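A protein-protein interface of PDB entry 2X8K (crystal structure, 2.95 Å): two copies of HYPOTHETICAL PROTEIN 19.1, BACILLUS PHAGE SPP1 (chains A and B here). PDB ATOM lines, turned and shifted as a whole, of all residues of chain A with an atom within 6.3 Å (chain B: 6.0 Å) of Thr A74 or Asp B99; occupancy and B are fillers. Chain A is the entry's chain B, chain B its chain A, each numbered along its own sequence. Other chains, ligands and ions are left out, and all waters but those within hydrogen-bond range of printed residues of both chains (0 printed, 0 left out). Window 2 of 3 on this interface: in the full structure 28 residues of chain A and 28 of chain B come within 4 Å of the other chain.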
ATOM      1  N   THR A  72       5.234  18.171   1.350  1.00  0.00           N
ATOM      2  CA  THR A  72       4.546  18.803   0.224  1.00  0.00           C
ATOM      3  C   THR A  72       3.650  17.782  -0.489  1.00  0.00           C
ATOM      4  O   THR A  72       3.824  16.573  -0.339  1.00  0.00           O
ATOM      5  CB  THR A  72       5.531  19.403  -0.799  1.00  0.00           C
ATOM      6  OG1 THR A  72       5.437  18.683  -2.036  1.00  0.00           O
ATOM      7  CG2 THR A  72       6.957  19.321  -0.278  1.00  0.00           C
ATOM      8  N   GLU A  73       2.696  18.291  -1.266  1.00  0.00           N
ATOM      9  CA  GLU A  73       1.782  17.470  -2.051  1.00  0.00           C
ATOM     10  C   GLU A  73       2.408  16.974  -3.335  1.00  0.00           C
ATOM     11  O   GLU A  73       2.294  15.786  -3.632  1.00  0.00           O
ATOM     12  CB  GLU A  73       0.446  18.178  -2.314  1.00  0.00           C
ATOM     13  CG  GLU A  73      -0.748  17.497  -1.645  1.00  0.00           C
ATOM     14  CD  GLU A  73      -1.010  16.025  -1.948  1.00  0.00           C
ATOM     15  OE1 GLU A  73      -1.288  15.267  -0.989  1.00  0.00           O
ATOM     16  OE2 GLU A  73      -0.947  15.626  -3.136  1.00  0.00           O
ATOM     17  N   THR A  74       3.111  17.853  -4.063  1.00  0.00           N
ATOM     18  CA  THR A  74       3.810  17.500  -5.306  1.00  0.00           C
ATOM     19  C   THR A  74       4.935  16.496  -5.048  1.00  0.00           C
ATOM     20  O   THR A  74       5.207  15.630  -5.886  1.00  0.00           O
ATOM     21  CB  THR A  74       4.368  18.745  -5.960  1.00  0.00           C
ATOM     22  OG1 THR A  74       3.411  19.807  -5.835  1.00  0.00           O
ATOM     23  CG2 THR A  74       4.744  18.510  -7.417  1.00  0.00           C
ATOM     24  N   ASP A  75       5.593  16.626  -3.883  1.00  0.00           N
ATOM     25  CA  ASP A  75       6.662  15.758  -3.433  1.00  0.00           C
ATOM     26  C   ASP A  75       6.110  14.356  -3.271  1.00  0.00           C
ATOM     27  O   ASP A  75       6.728  13.415  -3.759  1.00  0.00           O
ATOM     28  CB  ASP A  75       7.234  16.301  -2.126  1.00  0.00           C
ATOM     29  CG  ASP A  75       8.286  17.417  -2.243  1.00  0.00           C
ATOM     30  OD1 ASP A  75       8.173  18.285  -3.180  1.00  0.00           O
ATOM     31  OD2 ASP A  75       9.157  17.497  -1.350  1.00  0.00           O
ATOM     32  N   LEU A  76       4.896  14.220  -2.687  1.00  0.00           N
ATOM     33  CA  LEU A  76       4.217  12.933  -2.540  1.00  0.00           C
ATOM     34  C   LEU A  76       3.891  12.312  -3.907  1.00  0.00           C
ATOM     35  O   LEU A  76       4.137  11.119  -4.093  1.00  0.00           O
ATOM     36  CB  LEU A  76       2.937  13.078  -1.693  1.00  0.00           C
ATOM     37  CG  LEU A  76       2.027  11.807  -1.584  1.00  0.00           C
ATOM     38  CD1 LEU A  76       2.646  10.725  -0.717  1.00  0.00           C
ATOM     39  CD2 LEU A  76       0.656  12.153  -1.057  1.00  0.00           C
ATOM     40  N   ARG A  77       3.320  13.119  -4.849  1.00  0.00           N
ATOM     41  CA  ARG A  77       2.953  12.653  -6.191  1.00  0.00           C
ATOM     42  C   ARG A  77       4.175  12.101  -6.900  1.00  0.00           C
ATOM     43  O   ARG A  77       4.091  11.041  -7.540  1.00  0.00           O
ATOM     44  CB  ARG A  77       2.352  13.755  -7.060  1.00  0.00           C
ATOM     45  CG  ARG A  77       1.192  14.538  -6.490  1.00  0.00           C
ATOM     46  CD  ARG A  77      -0.148  13.964  -6.871  1.00  0.00           C
ATOM     47  NE  ARG A  77      -0.561  12.972  -5.888  1.00  0.00           N
ATOM     48  CZ  ARG A  77      -0.465  11.674  -6.090  1.00  0.00           C
ATOM     49  NH1 ARG A  77      -0.829  10.822  -5.141  1.00  0.00           N
ATOM     50  NH2 ARG A  77       0.032  11.208  -7.233  1.00  0.00           N
ATOM     51  N   ARG A  78       5.313  12.803  -6.762  1.00  0.00           N
ATOM     52  CA  ARG A  78       6.572  12.399  -7.367  1.00  0.00           C
ATOM     53  C   ARG A  78       7.203  11.165  -6.715  1.00  0.00           C
ATOM     54  O   ARG A  78       7.833  10.382  -7.420  1.00  0.00           O
ATOM     55  CB  ARG A  78       7.531  13.584  -7.513  1.00  0.00           C
ATOM     56  CG  ARG A  78       7.258  14.345  -8.798  1.00  0.00           C
ATOM     57  CD  ARG A  78       7.394  15.820  -8.609  1.00  0.00           C
ATOM     58  NE  ARG A  78       6.720  16.566  -9.677  1.00  0.00           N
ATOM     59  CZ  ARG A  78       7.301  17.494 -10.437  1.00  0.00           C
ATOM     60  NH1 ARG A  78       8.586  17.799 -10.264  1.00  0.00           N
ATOM     61  NH2 ARG A  78       6.603  18.121 -11.376  1.00  0.00           N
ATOM     62  N   ARG A  79       6.979  10.958  -5.403  1.00  0.00           N
ATOM     63  CA  ARG A  79       7.502   9.781  -4.707  1.00  0.00           C
ATOM     64  C   ARG A  79       6.784   8.551  -5.236  1.00  0.00           C
ATOM     65  O   ARG A  79       7.442   7.563  -5.562  1.00  0.00           O
ATOM     66  CB  ARG A  79       7.326   9.878  -3.177  1.00  0.00           C
ATOM     67  CG  ARG A  79       8.276  10.849  -2.477  1.00  0.00           C
ATOM     68  CD  ARG A  79       8.102  10.909  -0.956  1.00  0.00           C
ATOM     69  NE  ARG A  79       8.741   9.771  -0.273  1.00  0.00           N
ATOM     70  CZ  ARG A  79      10.030   9.710   0.075  1.00  0.00           C
ATOM     71  NH1 ARG A  79      10.847  10.723  -0.190  1.00  0.00           N
ATOM     72  NH2 ARG A  79      10.508   8.637   0.689  1.00  0.00           N
ATOM     73  N   PHE B  10      -7.192  24.369  -5.143  1.00  0.00           N
ATOM     74  CA  PHE B  10      -6.765  23.265  -5.979  1.00  0.00           C
ATOM     75  C   PHE B  10      -7.500  23.348  -7.312  1.00  0.00           C
ATOM     76  O   PHE B  10      -8.732  23.241  -7.339  1.00  0.00           O
ATOM     77  CB  PHE B  10      -7.093  21.938  -5.284  1.00  0.00           C
ATOM     78  CG  PHE B  10      -6.810  20.714  -6.112  1.00  0.00           C
ATOM     79  CD1 PHE B  10      -5.545  20.140  -6.122  1.00  0.00           C
ATOM     80  CD2 PHE B  10      -7.816  20.112  -6.858  1.00  0.00           C
ATOM     81  CE1 PHE B  10      -5.278  19.009  -6.891  1.00  0.00           C
ATOM     82  CE2 PHE B  10      -7.554  18.960  -7.606  1.00  0.00           C
ATOM     83  CZ  PHE B  10      -6.281  18.424  -7.625  1.00  0.00           C
ATOM     84  N   THR B  11      -6.762  23.533  -8.412  1.00  0.00           N
ATOM     85  CA  THR B  11      -7.424  23.573  -9.712  1.00  0.00           C
ATOM     86  C   THR B  11      -7.237  22.311 -10.568  1.00  0.00           C
ATOM     87  O   THR B  11      -6.155  21.712 -10.585  1.00  0.00           O
ATOM     88  CB  THR B  11      -7.161  24.864 -10.466  1.00  0.00           C
ATOM     89  OG1 THR B  11      -5.764  24.997 -10.633  1.00  0.00           O
ATOM     90  CG2 THR B  11      -7.721  26.074  -9.761  1.00  0.00           C
ATOM     91  N   ARG B  31      -4.370   8.217  -9.035  1.00  0.00           N
ATOM     92  CA  ARG B  31      -2.964   8.534  -9.335  1.00  0.00           C
ATOM     93  C   ARG B  31      -1.958   8.118  -8.229  1.00  0.00           C
ATOM     94  O   ARG B  31      -1.053   8.857  -7.845  1.00  0.00           O
ATOM     95  CB  ARG B  31      -2.798   9.956  -9.841  1.00  0.00           C
ATOM     96  CG  ARG B  31      -3.247  11.000  -8.862  1.00  0.00           C
ATOM     97  CD  ARG B  31      -3.924  12.112  -9.581  1.00  0.00           C
ATOM     98  NE  ARG B  31      -3.535  13.415  -9.033  1.00  0.00           N
ATOM     99  CZ  ARG B  31      -3.799  13.835  -7.796  1.00  0.00           C
ATOM    100  NH1 ARG B  31      -4.392  13.031  -6.924  1.00  0.00           N
ATOM    101  NH2 ARG B  31      -3.434  15.044  -7.411  1.00  0.00           N
ATOM    102  N   PHE B  97      -3.777  18.749 -12.825  1.00  0.00           N
ATOM    103  CA  PHE B  97      -4.096  19.086 -11.443  1.00  0.00           C
ATOM    104  C   PHE B  97      -3.029  20.033 -10.920  1.00  0.00           C
ATOM    105  O   PHE B  97      -1.858  19.841 -11.230  1.00  0.00           O
ATOM    106  CB  PHE B  97      -4.180  17.833 -10.576  1.00  0.00           C
ATOM    107  CG  PHE B  97      -5.152  16.808 -11.097  1.00  0.00           C
ATOM    108  CD1 PHE B  97      -4.703  15.697 -11.805  1.00  0.00           C
ATOM    109  CD2 PHE B  97      -6.513  16.942 -10.868  1.00  0.00           C
ATOM    110  CE1 PHE B  97      -5.605  14.753 -12.300  1.00  0.00           C
ATOM    111  CE2 PHE B  97      -7.408  15.981 -11.326  1.00  0.00           C
ATOM    112  CZ  PHE B  97      -6.950  14.891 -12.044  1.00  0.00           C
ATOM    113  N   SER B  98      -3.443  21.074 -10.163  1.00  0.00           N
ATOM    114  CA  SER B  98      -2.542  22.072  -9.606  1.00  0.00           C
ATOM    115  C   SER B  98      -1.505  21.477  -8.664  1.00  0.00           C
ATOM    116  O   SER B  98      -0.390  21.975  -8.628  1.00  0.00           O
ATOM    117  CB  SER B  98      -3.316  23.191  -8.918  1.00  0.00           C
ATOM    118  OG  SER B  98      -3.971  22.749  -7.743  1.00  0.00           O
ATOM    119  N   ASP B  99      -1.841  20.402  -7.931  1.00  0.00           N
ATOM    120  CA  ASP B  99      -0.892  19.760  -7.016  1.00  0.00           C
ATOM    121  C   ASP B  99       0.223  19.041  -7.752  1.00  0.00           C
ATOM    122  O   ASP B  99       1.263  18.757  -7.164  1.00  0.00           O
ATOM    123  CB  ASP B  99      -1.582  18.845  -5.980  1.00  0.00           C
ATOM    124  CG  ASP B  99      -2.283  17.613  -6.500  1.00  0.00           C
ATOM    125  OD1 ASP B  99      -2.380  17.452  -7.751  1.00  0.00           O
ATOM    126  OD2 ASP B  99      -2.770  16.822  -5.666  1.00  0.00           O
ATOM    127  N   GLU B 100       0.018  18.744  -9.034  1.00  0.00           N
ATOM    128  CA  GLU B 100       1.072  18.116  -9.787  1.00  0.00           C
ATOM    129  C   GLU B 100       1.421  18.816 -11.072  1.00  0.00           C
ATOM    130  O   GLU B 100       0.988  18.409 -12.155  1.00  0.00           O
ATOM    131  CB  GLU B 100       0.977  16.595  -9.850  1.00  0.00           C
ATOM    132  CG  GLU B 100      -0.149  16.041 -10.683  1.00  0.00           C
ATOM    133  CD  GLU B 100      -0.182  14.535 -10.656  1.00  0.00           C
ATOM    134  OE1 GLU B 100       0.909  13.908 -10.663  1.00  0.00           O
ATOM    135  OE2 GLU B 100      -1.307  13.986 -10.612  1.00  0.00           O
ATOM    136  N   PRO B 101       2.198  19.921 -10.942  1.00  0.00           N
ATOM    137  CA  PRO B 101       2.619  20.667 -12.125  1.00  0.00           C
ATOM    138  C   PRO B 101       3.611  19.859 -12.961  1.00  0.00           C
ATOM    139  O   PRO B 101       4.216  18.882 -12.477  1.00  0.00           O
ATOM    140  CB  PRO B 101       3.279  21.900 -11.514  1.00  0.00           C
ATOM    141  CG  PRO B 101       3.849  21.406 -10.221  1.00  0.00           C
ATOM    142  CD  PRO B 101       2.788  20.510  -9.716  1.00  0.00           C
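The side-chain carboxylate of Glu A73 lies within salt-bridge range of the guanidinium group of Arg A77.
The guanidinium group (NH2) of Arg B31 lies within salt-bridge range of the side-chain carboxylate (OD2) of Asp B99 (2.6 Å).
The side-chain hydroxyl (OG1) of Thr A72 sits at hydrogen-bond distance from the backbone NH (N) of Thr A74, 3.2 Å away.
NE of Arg B31 is in salt-bridge range of OE2 of Glu B100, 2.8 Å away.
Thr A74 touches Pro B101.
Glu B100 touches Arg A77.
Of the 8 printed residues of chain B, 4 touch a printed residue of chain A.
Hydrophobic or aromatic side chains of chain B within 4 Å of the printed part of chain A: Pro B101.
Printed residues of chain A that touch a printed residue of chain B: Glu A73, Thr A74, Arg A77 and Arg A78.
Of the printed residues of chain B, Glu A73 touches Asp B99 (3.3 Å).
Of the printed residues of chain B, Arg A78 touches Pro B101 (2.7 Å).
Of the printed residues of chain A, Arg B31 touches Arg A77.
Of chain A, only Glu A73 (3.3 Å) and Thr A74 (2.7 Å) come within 4 Å of Asp B99.
The nearest residue of chain B that does not touch Thr A74 is Glu B100 (4.4 Å).
The nearest printed residue of chain B that does not touch Arg A77 is Asp B99 (4.1 Å).
No position is printed for both chains.
The backbone carbonyl oxygen (O) of Asp B99 is in hydrogen-bond range of the side-chain hydroxyl (OG1) of Thr A74 (2.7 Å).
NH2 of Arg A77 lies within hydrogen-bond range of O of Arg B31.
The side-chain carboxylate (OD2) of Asp B99 sits close to the side-chain carboxylate (OE2) of Glu A73 (3.3 Å).
The backbone carbonyl oxygen (O) of Pro B101 is in hydrogen-bond range of the guanidinium group (NH2) of Arg A78, at 2.7 Å.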
